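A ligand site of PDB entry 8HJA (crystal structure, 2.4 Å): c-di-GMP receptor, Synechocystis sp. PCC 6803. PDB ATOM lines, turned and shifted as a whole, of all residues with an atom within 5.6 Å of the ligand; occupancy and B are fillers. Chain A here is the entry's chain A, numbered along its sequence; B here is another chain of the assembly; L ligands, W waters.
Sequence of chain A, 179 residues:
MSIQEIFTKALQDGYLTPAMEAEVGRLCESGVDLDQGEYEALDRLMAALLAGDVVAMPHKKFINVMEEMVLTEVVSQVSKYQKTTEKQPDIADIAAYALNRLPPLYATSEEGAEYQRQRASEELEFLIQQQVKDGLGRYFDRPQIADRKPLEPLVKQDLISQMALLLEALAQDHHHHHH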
ATOM      1  N   ASP A  90      14.215   9.495   8.551  1.00  0.00           N
ATOM      2  CA  ASP A  90      14.989   8.271   8.467  1.00  0.00           C
ATOM      3  C   ASP A  90      16.252   8.587   7.693  1.00  0.00           C
ATOM      4  O   ASP A  90      16.213   8.752   6.484  1.00  0.00           O
ATOM      5  CB  ASP A  90      14.124   7.177   7.853  1.00  0.00           C
ATOM      6  CG  ASP A  90      14.629   5.758   8.040  1.00  0.00           C
ATOM      7  OD1 ASP A  90      15.781   5.451   7.630  1.00  0.00           O
ATOM      8  OD2 ASP A  90      13.855   4.937   8.575  1.00  0.00           O
ATOM      9  N   ALA A  92      18.882   6.734   7.189  1.00  0.00           N
ATOM     10  CA  ALA A  92      19.343   5.605   6.391  1.00  0.00           C
ATOM     11  C   ALA A  92      18.641   5.647   5.047  1.00  0.00           C
ATOM     12  O   ALA A  92      19.322   5.531   4.034  1.00  0.00           O
ATOM     13  CB  ALA A  92      19.061   4.282   7.092  1.00  0.00           C
ATOM     14  N   ASP A  93      17.318   5.868   5.061  1.00  0.00           N
ATOM     15  CA  ASP A  93      16.470   5.960   3.865  1.00  0.00           C
ATOM     16  C   ASP A  93      16.957   7.055   2.911  1.00  0.00           C
ATOM     17  O   ASP A  93      17.073   6.860   1.713  1.00  0.00           O
ATOM     18  CB  ASP A  93      15.024   6.331   4.203  1.00  0.00           C
ATOM     19  CG  ASP A  93      14.068   5.199   4.519  1.00  0.00           C
ATOM     20  OD1 ASP A  93      14.415   3.993   4.211  1.00  0.00           O
ATOM     21  OD2 ASP A  93      12.949   5.523   5.036  1.00  0.00           O
ATOM     22  N   ILE A  94      17.259   8.212   3.480  1.00  0.00           N
ATOM     23  CA  ILE A  94      17.661   9.364   2.712  1.00  0.00           C
ATOM     24  C   ILE A  94      19.036   9.112   2.104  1.00  0.00           C
ATOM     25  O   ILE A  94      19.227   9.495   0.966  1.00  0.00           O
ATOM     26  CB  ILE A  94      17.620  10.644   3.586  1.00  0.00           C
ATOM     27  CG1 ILE A  94      16.201  10.908   4.081  1.00  0.00           C
ATOM     28  CG2 ILE A  94      18.173  11.857   2.864  1.00  0.00           C
ATOM     29  CD1 ILE A  94      16.137  12.026   5.093  1.00  0.00           C
ATOM     30  N   ALA A  96      20.750   6.199   1.600  1.00  0.00           N
ATOM     31  CA  ALA A  96      20.715   5.117   0.636  1.00  0.00           C
ATOM     32  C   ALA A  96      20.117   5.563  -0.723  1.00  0.00           C
ATOM     33  O   ALA A  96      20.640   5.194  -1.784  1.00  0.00           O
ATOM     34  CB  ALA A  96      19.989   3.947   1.265  1.00  0.00           C
ATOM     35  N   TYR A  97      19.046   6.386  -0.710  1.00  0.00           N
ATOM     36  CA  TYR A  97      18.461   6.942  -1.944  1.00  0.00           C
ATOM     37  C   TYR A  97      19.559   7.686  -2.689  1.00  0.00           C
ATOM     38  O   TYR A  97      19.806   7.446  -3.864  1.00  0.00           O
ATOM     39  CB  TYR A  97      17.266   7.873  -1.681  1.00  0.00           C
ATOM     40  CG  TYR A  97      16.779   8.593  -2.914  1.00  0.00           C
ATOM     41  CD1 TYR A  97      17.431   9.729  -3.364  1.00  0.00           C
ATOM     42  CD2 TYR A  97      15.721   8.110  -3.679  1.00  0.00           C
ATOM     43  CE1 TYR A  97      17.046  10.392  -4.520  1.00  0.00           C
ATOM     44  CE2 TYR A  97      15.357   8.740  -4.861  1.00  0.00           C
ATOM     45  CZ  TYR A  97      16.009   9.890  -5.282  1.00  0.00           C
ATOM     46  OH  TYR A  97      15.664  10.603  -6.447  1.00  0.00           O
ATOM     47  N   ASN A 100      22.735   5.620  -4.097  1.00  0.00           N
ATOM     48  CA  ASN A 100      22.395   4.982  -5.354  1.00  0.00           C
ATOM     49  C   ASN A 100      22.436   5.908  -6.564  1.00  0.00           C
ATOM     50  O   ASN A 100      22.418   5.400  -7.678  1.00  0.00           O
ATOM     51  CB  ASN A 100      21.028   4.304  -5.199  1.00  0.00           C
ATOM     52  CG  ASN A 100      21.185   2.928  -4.563  1.00  0.00           C
ATOM     53  OD1 ASN A 100      22.293   2.393  -4.552  1.00  0.00           O
ATOM     54  ND2 ASN A 100      20.098   2.371  -4.050  1.00  0.00           N
ATOM     55  N   ARG A 101      22.534   7.243  -6.390  1.00  0.00           N
ATOM     56  CA  ARG A 101      22.547   8.170  -7.518  1.00  0.00           C
ATOM     57  C   ARG A 101      23.816   9.022  -7.525  1.00  0.00           C
ATOM     58  O   ARG A 101      23.853  10.055  -8.174  1.00  0.00           O
ATOM     59  CB  ARG A 101      21.295   9.040  -7.507  1.00  0.00           C
ATOM     60  CG  ARG A 101      20.056   8.240  -7.823  1.00  0.00           C
ATOM     61  CD  ARG A 101      18.885   8.654  -6.983  1.00  0.00           C
ATOM     62  NE  ARG A 101      17.745   7.822  -7.317  1.00  0.00           N
ATOM     63  CZ  ARG A 101      17.389   6.711  -6.677  1.00  0.00           C
ATOM     64  NH1 ARG A 101      18.067   6.277  -5.646  1.00  0.00           N
ATOM     65  NH2 ARG A 101      16.315   6.042  -7.079  1.00  0.00           N
ATOM     66  N   ARG A 138      11.628  12.607  -1.117  1.00  0.00           N
ATOM     67  CA  ARG A 138      10.993  11.301  -1.179  1.00  0.00           C
ATOM     68  C   ARG A 138      10.642  10.731   0.206  1.00  0.00           C
ATOM     69  O   ARG A 138       9.645  10.048   0.352  1.00  0.00           O
ATOM     70  CB  ARG A 138      11.945  10.319  -1.872  1.00  0.00           C
ATOM     71  CG  ARG A 138      11.314   9.454  -2.934  1.00  0.00           C
ATOM     72  CD  ARG A 138      11.284  10.122  -4.293  1.00  0.00           C
ATOM     73  NE  ARG A 138      11.544   9.150  -5.364  1.00  0.00           N
ATOM     74  CZ  ARG A 138      11.821   9.464  -6.626  1.00  0.00           C
ATOM     75  NH1 ARG A 138      11.782  10.724  -7.044  1.00  0.00           N
ATOM     76  NH2 ARG A 138      12.138   8.505  -7.487  1.00  0.00           N
ATOM     77  N   TYR A 139      11.511  10.975   1.217  1.00  0.00           N
ATOM     78  CA  TYR A 139      11.177  10.637   2.596  1.00  0.00           C
ATOM     79  C   TYR A 139       9.920  11.396   3.059  1.00  0.00           C
ATOM     80  O   TYR A 139       8.994  10.783   3.587  1.00  0.00           O
ATOM     81  CB  TYR A 139      12.345  10.853   3.582  1.00  0.00           C
ATOM     82  CG  TYR A 139      11.901  10.622   5.008  1.00  0.00           C
ATOM     83  CD1 TYR A 139      11.279  11.622   5.719  1.00  0.00           C
ATOM     84  CD2 TYR A 139      11.945   9.365   5.578  1.00  0.00           C
ATOM     85  CE1 TYR A 139      10.770  11.407   6.993  1.00  0.00           C
ATOM     86  CE2 TYR A 139      11.446   9.118   6.845  1.00  0.00           C
ATOM     87  CZ  TYR A 139      10.855  10.141   7.563  1.00  0.00           C
ATOM     88  OH  TYR A 139      10.386   9.947   8.842  1.00  0.00           O
ATOM     89  N   ARG A 142       6.981   9.949   1.516  1.00  0.00           N
ATOM     90  CA  ARG A 142       6.570   8.594   1.902  1.00  0.00           C
ATOM     91  C   ARG A 142       7.462   8.089   3.039  1.00  0.00           C
ATOM     92  O   ARG A 142       8.317   7.251   2.822  1.00  0.00           O
ATOM     93  CB  ARG A 142       6.585   7.667   0.690  1.00  0.00           C
ATOM     94  CG  ARG A 142       5.352   6.774   0.561  1.00  0.00           C
ATOM     95  CD  ARG A 142       5.560   5.422  -0.084  1.00  0.00           C
ATOM     96  NE  ARG A 142       6.631   5.421  -1.056  1.00  0.00           N
ATOM     97  CZ  ARG A 142       7.055   4.352  -1.731  1.00  0.00           C
ATOM     98  NH1 ARG A 142       6.465   3.172  -1.570  1.00  0.00           N
ATOM     99  NH2 ARG A 142       8.058   4.479  -2.590  1.00  0.00           N
ATOM    100  N   PRO A 143       7.273   8.564   4.287  1.00  0.00           N
ATOM    101  CA  PRO A 143       8.182   8.235   5.385  1.00  0.00           C
ATOM    102  C   PRO A 143       8.302   6.756   5.755  1.00  0.00           C
ATOM    103  O   PRO A 143       9.315   6.367   6.324  1.00  0.00           O
ATOM    104  CB  PRO A 143       7.638   9.041   6.591  1.00  0.00           C
ATOM    105  CG  PRO A 143       6.201   9.403   6.221  1.00  0.00           C
ATOM    106  CD  PRO A 143       6.184   9.481   4.711  1.00  0.00           C
ATOM    107  N   GLN A 144       7.253   5.991   5.449  1.00  0.00           N
ATOM    108  CA  GLN A 144       7.160   4.568   5.745  1.00  0.00           C
ATOM    109  C   GLN A 144       6.642   3.831   4.518  1.00  0.00           C
ATOM    110  O   GLN A 144       5.478   4.007   4.159  1.00  0.00           O
ATOM    111  CB  GLN A 144       6.178   4.295   6.899  1.00  0.00           C
ATOM    112  CG  GLN A 144       6.798   4.491   8.279  1.00  0.00           C
ATOM    113  CD  GLN A 144       5.846   5.224   9.194  1.00  0.00           C
ATOM    114  OE1 GLN A 144       6.019   6.412   9.458  1.00  0.00           O
ATOM    115  NE2 GLN A 144       4.819   4.530   9.665  1.00  0.00           N
ATOM    116  N   ILE A 145       7.524   3.022   3.901  1.00  0.00           N
ATOM    117  CA  ILE A 145       7.163   2.126   2.806  1.00  0.00           C
ATOM    118  C   ILE A 145       6.577   0.864   3.415  1.00  0.00           C
ATOM    119  O   ILE A 145       7.153   0.332   4.353  1.00  0.00           O
ATOM    120  CB  ILE A 145       8.360   1.773   1.896  1.00  0.00           C
ATOM    121  CG1 ILE A 145       9.160   2.998   1.418  1.00  0.00           C
ATOM    122  CG2 ILE A 145       7.915   0.914   0.726  1.00  0.00           C
ATOM    123  CD1 ILE A 145      10.431   2.644   0.627  1.00  0.00           C
ATOM    124  N   ARG A 148       8.289  -3.651   4.123  1.00  0.00           N
ATOM    125  CA  ARG A 148       9.674  -3.766   4.527  1.00  0.00           C
ATOM    126  C   ARG A 148      10.082  -4.144   5.952  1.00  0.00           C
ATOM    127  O   ARG A 148       9.653  -3.506   6.907  1.00  0.00           O
ATOM    128  CB  ARG A 148      10.080  -2.371   4.014  1.00  0.00           C
ATOM    129  CG  ARG A 148       9.741  -2.067   2.558  1.00  0.00           C
ATOM    130  CD  ARG A 148      10.786  -2.492   1.532  1.00  0.00           C
ATOM    131  NE  ARG A 148      10.489  -2.171   0.123  1.00  0.00           N
ATOM    132  CZ  ARG A 148       9.493  -2.707  -0.605  1.00  0.00           C
ATOM    133  NH1 ARG A 148       8.610  -3.516  -0.048  1.00  0.00           N
ATOM    134  NH2 ARG A 148       9.401  -2.453  -1.888  1.00  0.00           N
ATOM    135  N   TYR B 106      22.400   0.127  -2.995  1.00  0.00           N
ATOM    136  CA  TYR B 106      22.181   0.359  -1.547  1.00  0.00           C
ATOM    137  C   TYR B 106      20.737   0.031  -1.151  1.00  0.00           C
ATOM    138  O   TYR B 106      19.800   0.563  -1.784  1.00  0.00           O
ATOM    139  CB  TYR B 106      22.534   1.800  -1.175  1.00  0.00           C
ATOM    140  CG  TYR B 106      24.008   2.022  -0.958  1.00  0.00           C
ATOM    141  CD1 TYR B 106      24.843   2.360  -2.006  1.00  0.00           C
ATOM    142  CD2 TYR B 106      24.569   1.895   0.302  1.00  0.00           C
ATOM    143  CE1 TYR B 106      26.196   2.564  -1.824  1.00  0.00           C
ATOM    144  CE2 TYR B 106      25.923   2.092   0.506  1.00  0.00           C
ATOM    145  CZ  TYR B 106      26.737   2.428  -0.552  1.00  0.00           C
ATOM    146  OH  TYR B 106      28.081   2.624  -0.358  1.00  0.00           O
ATOM    147  N   ALA B 107      20.569  -0.816  -0.133  1.00  0.00           N
ATOM    148  CA  ALA B 107      19.227  -1.116   0.368  1.00  0.00           C
ATOM    149  C   ALA B 107      19.232  -1.002   1.879  1.00  0.00           C
ATOM    150  O   ALA B 107      20.311  -1.007   2.497  1.00  0.00           O
ATOM    151  CB  ALA B 107      18.765  -2.506   0.011  1.00  0.00           C
ATOM    152  N   THR B 108      18.007  -0.928   2.429  1.00  0.00           N
ATOM    153  CA  THR B 108      17.808  -0.771   3.847  1.00  0.00           C
ATOM    154  C   THR B 108      16.798  -1.794   4.411  1.00  0.00           C
ATOM    155  O   THR B 108      16.626  -1.860   5.631  1.00  0.00           O
ATOM    156  CB  THR B 108      17.309   0.647   4.166  1.00  0.00           C
ATOM    157  OG1 THR B 108      16.075   0.796   3.449  1.00  0.00           O
ATOM    158  CG2 THR B 108      18.295   1.733   3.816  1.00  0.00           C
ATOM    159  N   SER B 109      16.120  -2.532   3.523  1.00  0.00           N
ATOM    160  CA  SER B 109      15.164  -3.567   3.874  1.00  0.00           C
ATOM    161  C   SER B 109      15.582  -4.895   3.230  1.00  0.00           C
ATOM    162  O   SER B 109      16.405  -4.911   2.318  1.00  0.00           O
ATOM    163  CB  SER B 109      13.775  -3.194   3.440  1.00  0.00           C
ATOM    164  OG  SER B 109      13.616  -3.413   2.051  1.00  0.00           O
ATOM    165  N   GLU B 111      13.578  -6.928   1.590  1.00  0.00           N
ATOM    166  CA  GLU B 111      12.928  -6.908   0.299  1.00  0.00           C
ATOM    167  C   GLU B 111      13.768  -6.125  -0.688  1.00  0.00           C
ATOM    168  O   GLU B 111      13.929  -6.544  -1.832  1.00  0.00           O
ATOM    169  CB  GLU B 111      11.552  -6.276   0.421  1.00  0.00           C
ATOM    170  CG  GLU B 111      10.523  -7.201   1.031  1.00  0.00           C
ATOM    171  CD  GLU B 111      10.509  -7.238   2.546  1.00  0.00           C
ATOM    172  OE1 GLU B 111      11.450  -6.652   3.146  1.00  0.00           O
ATOM    173  OE2 GLU B 111       9.544  -7.824   3.120  1.00  0.00           O
ATOM    174  N   GLY B 112      14.307  -4.972  -0.236  1.00  0.00           N
ATOM    175  CA  GLY B 112      15.039  -4.086  -1.124  1.00  0.00           C
ATOM    176  C   GLY B 112      16.324  -4.760  -1.572  1.00  0.00           C
ATOM    177  O   GLY B 112      16.678  -4.682  -2.738  1.00  0.00           O
ATOM    178  N   ALA B 113      16.963  -5.428  -0.605  1.00  0.00           N
ATOM    179  CA  ALA B 113      18.139  -6.257  -0.802  1.00  0.00           C
ATOM    180  C   ALA B 113      17.843  -7.387  -1.781  1.00  0.00           C
ATOM    181  O   ALA B 113      18.630  -7.654  -2.673  1.00  0.00           O
ATOM    182  CB  ALA B 113      18.607  -6.757   0.549  1.00  0.00           C
ATOM    183  N   TYR B 115      15.648  -7.433  -4.223  1.00  0.00           N
ATOM    184  CA  TYR B 115      15.560  -6.787  -5.526  1.00  0.00           C
ATOM    185  C   TYR B 115      16.939  -6.446  -6.095  1.00  0.00           C
ATOM    186  O   TYR B 115      17.165  -6.597  -7.282  1.00  0.00           O
ATOM    187  CB  TYR B 115      14.775  -5.483  -5.445  1.00  0.00           C
ATOM    188  CG  TYR B 115      13.292  -5.622  -5.259  1.00  0.00           C
ATOM    189  CD1 TYR B 115      12.519  -6.214  -6.238  1.00  0.00           C
ATOM    190  CD2 TYR B 115      12.660  -5.162  -4.118  1.00  0.00           C
ATOM    191  CE1 TYR B 115      11.134  -6.338  -6.098  1.00  0.00           C
ATOM    192  CE2 TYR B 115      11.286  -5.283  -3.959  1.00  0.00           C
ATOM    193  CZ  TYR B 115      10.523  -5.866  -4.950  1.00  0.00           C
ATOM    194  OH  TYR B 115       9.168  -6.020  -4.806  1.00  0.00           O
ATOM    195  N   GLN B 116      17.859  -5.973  -5.243  1.00  0.00           N
ATOM    196  CA  GLN B 116      19.181  -5.585  -5.696  1.00  0.00           C
ATOM    197  C   GLN B 116      19.986  -6.836  -6.090  1.00  0.00           C
ATOM    198  O   GLN B 116      20.737  -6.799  -7.039  1.00  0.00           O
ATOM    199  CB  GLN B 116      19.891  -4.671  -4.654  1.00  0.00           C
ATOM    200  CG  GLN B 116      19.212  -3.313  -4.371  1.00  0.00           C
ATOM    201  CD  GLN B 116      19.385  -2.286  -5.468  1.00  0.00           C
ATOM    202  OE1 GLN B 116      19.353  -2.634  -6.658  1.00  0.00           O
ATOM    203  NE2 GLN B 116      19.629  -1.032  -5.114  1.00  0.00           N
HETATM  204  P1  LIG L   1      16.313   2.879  -4.579  1.00  0.00           P
HETATM  205  O1  LIG L   1      14.998   3.134  -5.260  1.00  0.00           O
HETATM  206  O2  LIG L   1      17.570   3.566  -5.056  1.00  0.00           O
HETATM  207  O3  LIG L   1      15.976   3.145  -3.031  1.00  0.00           O
HETATM  208  C1  LIG L   1      17.125   3.061  -2.140  1.00  0.00           C
HETATM  209  C2  LIG L   1      16.655   3.285  -0.713  1.00  0.00           C
HETATM  210  O4  LIG L   1      16.162   4.647  -0.558  1.00  0.00           O
HETATM  211  C3  LIG L   1      15.489   2.411  -0.280  1.00  0.00           C
HETATM  212  O5  LIG L   1      15.977   1.141   0.087  1.00  0.00           O
HETATM  213  C4  LIG L   1      14.914   3.219   0.876  1.00  0.00           C
HETATM  214  O6  LIG L   1      15.583   3.057   2.097  1.00  0.00           O
HETATM  215  C5  LIG L   1      15.099   4.662   0.371  1.00  0.00           C
HETATM  216  N1  LIG L   1      13.893   5.213  -0.238  1.00  0.00           N
HETATM  217  C6  LIG L   1      13.582   5.263  -1.573  1.00  0.00           C
HETATM  218  N2  LIG L   1      12.377   5.741  -1.806  1.00  0.00           N
HETATM  219  C7  LIG L   1      11.872   6.041  -0.543  1.00  0.00           C
HETATM  220  C8  LIG L   1      10.646   6.618  -0.142  1.00  0.00           C
HETATM  221  O7  LIG L   1       9.699   6.968  -0.839  1.00  0.00           O
HETATM  222  N3  LIG L   1      10.526   6.718   1.232  1.00  0.00           N
HETATM  223  C9  LIG L   1      11.470   6.320   2.139  1.00  0.00           C
HETATM  224  N4  LIG L   1      11.146   6.524   3.422  1.00  0.00           N
HETATM  225  N5  LIG L   1      12.637   5.791   1.793  1.00  0.00           N
HETATM  226  C10 LIG L   1      12.787   5.694   0.437  1.00  0.00           C
HETATM  227  P2  LIG L   1      14.987  -0.116  -0.134  1.00  0.00           P
HETATM  228  O8  LIG L   1      13.556   0.105   0.277  1.00  0.00           O
HETATM  229  O9  LIG L   1      15.674  -1.233   0.609  1.00  0.00           O
HETATM  230  O10 LIG L   1      15.023  -0.430  -1.696  1.00  0.00           O
HETATM  231  C11 LIG L   1      16.343  -0.758  -2.198  1.00  0.00           C
HETATM  232  C12 LIG L   1      16.239  -0.860  -3.688  1.00  0.00           C
HETATM  233  O11 LIG L   1      15.313  -1.918  -4.003  1.00  0.00           O
HETATM  234  C13 LIG L   1      15.671   0.378  -4.382  1.00  0.00           C
HETATM  235  O12 LIG L   1      16.689   1.326  -4.711  1.00  0.00           O
HETATM  236  C14 LIG L   1      15.120  -0.236  -5.658  1.00  0.00           C
HETATM  237  O13 LIG L   1      16.145  -0.463  -6.583  1.00  0.00           O
HETATM  238  C15 LIG L   1      14.592  -1.576  -5.170  1.00  0.00           C
HETATM  239  N6  LIG L   1      13.170  -1.568  -4.887  1.00  0.00           N
HETATM  240  C16 LIG L   1      12.475  -1.029  -3.818  1.00  0.00           C
HETATM  241  N7  LIG L   1      11.174  -1.207  -3.905  1.00  0.00           N
HETATM  242  C17 LIG L   1      11.026  -1.894  -5.110  1.00  0.00           C
HETATM  243  C18 LIG L   1       9.853  -2.378  -5.740  1.00  0.00           C
HETATM  244  O14 LIG L   1       8.683  -2.277  -5.348  1.00  0.00           O
HETATM  245  N8  LIG L   1      10.174  -3.015  -6.945  1.00  0.00           N
HETATM  246  C19 LIG L   1      11.441  -3.176  -7.473  1.00  0.00           C
HETATM  247  N9  LIG L   1      11.564  -3.832  -8.639  1.00  0.00           N
HETATM  248  N10 LIG L   1      12.535  -2.738  -6.863  1.00  0.00           N
HETATM  249  C20 LIG L   1      12.241  -2.107  -5.708  1.00  0.00           C
HETATM  250  O   HOH W   1      18.492   3.044  -7.532  1.00  0.00           O
HETATM  251  O   HOH W   2      13.572   0.257   3.524  1.00  0.00           O
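Water W2 bridges OG1 of Thr 108 of chain B (2.6 Å) and O8 of the ligand (3.3 Å).
The backbone carbonyl oxygen (O) of Arg 138 lies close to an oxygen (O7) of the ligand (3.3 Å). O of Gly 112 of chain B lies close to O11 of the ligand (3.3 Å). Residues that only touch the ligand: Ala 96 (3.9 Å), Tyr 139 (3.7 Å), Ile 145 (3.9 Å), Tyr 106 of chain B (3.7 Å), Ala 107 of chain B (3.4 Å), Tyr 115 of chain B (3.4 Å) and Gln 116 of chain B (3.7 Å). Hydrophobic or aromatic side chains within 4 Å of the ligand: Ala 96, Tyr 97, Tyr 139, Ile 145, Ala 107 of chain B and Tyr 115 of chain B. Of the 24 residues printed, 18 come within 4 Å of the ligand. Along chain A the residues within 4 Å of the ligand span positions 93 to 148. The nearest printed residue that does not touch the ligand is Gln 144 (4.4 Å).
The side-chain carboxylate (OD1) of Asp 90 lies within hydrogen-bond range of the backbone NH (N) of Asp 93 (3.0 Å). O of Tyr 97 is in hydrogen-bond range of NH1 of Arg 101. The backbone NH (N) of Tyr 106 of chain B lies within hydrogen-bond range of the side-chain amide oxygen (OD1) of Asn 100 (2.8 Å). OG of Ser 109 of chain B lies within hydrogen-bond range of N of Gly 112 of chain B (2.9 Å).
The guanidinium group of Arg 148 is in salt-bridge range of an oxygen (O8) of the ligand, at 3.8 Å. The guanidinium group (NE) of Arg 142 lies within hydrogen-bond range of an oxygen (O7) of the ligand (3.4 Å). An oxygen (O2) of the ligand is in hydrogen-bond range of the side-chain amide nitrogen (ND2) of Asn 100, at 3.0 Å. The backbone NH of Ser 109 of chain B sits at hydrogen-bond distance from an oxygen (O9) of the ligand (3.2 Å). NH1 of Arg 101 is in salt-bridge range of O2 of the ligand (2.8 Å). OD1 of Asp 93 is in hydrogen-bond range of O6 of the ligand (2.6 Å). The side-chain hydroxyl (OG) of Ser 109 of chain B lies within hydrogen-bond range of an oxygen (O9) of the ligand, 3.3 Å away. The backbone carbonyl oxygen of Arg 142 is in hydrogen-bond range of a nitrogen (N3) of the ligand. The backbone carbonyl oxygen (O) of Pro 143 sits at hydrogen-bond distance from a nitrogen (N4) of the ligand. OG1 of Thr 108 of chain B lies within hydrogen-bond range of O6 of the ligand (2.7 Å). An oxygen (O9) of the ligand sits at hydrogen-bond distance from the backbone NH (N) of Thr 108 of chain B (3.0 Å). N of Tyr 97 sits at hydrogen-bond distance from O4 of the ligand.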
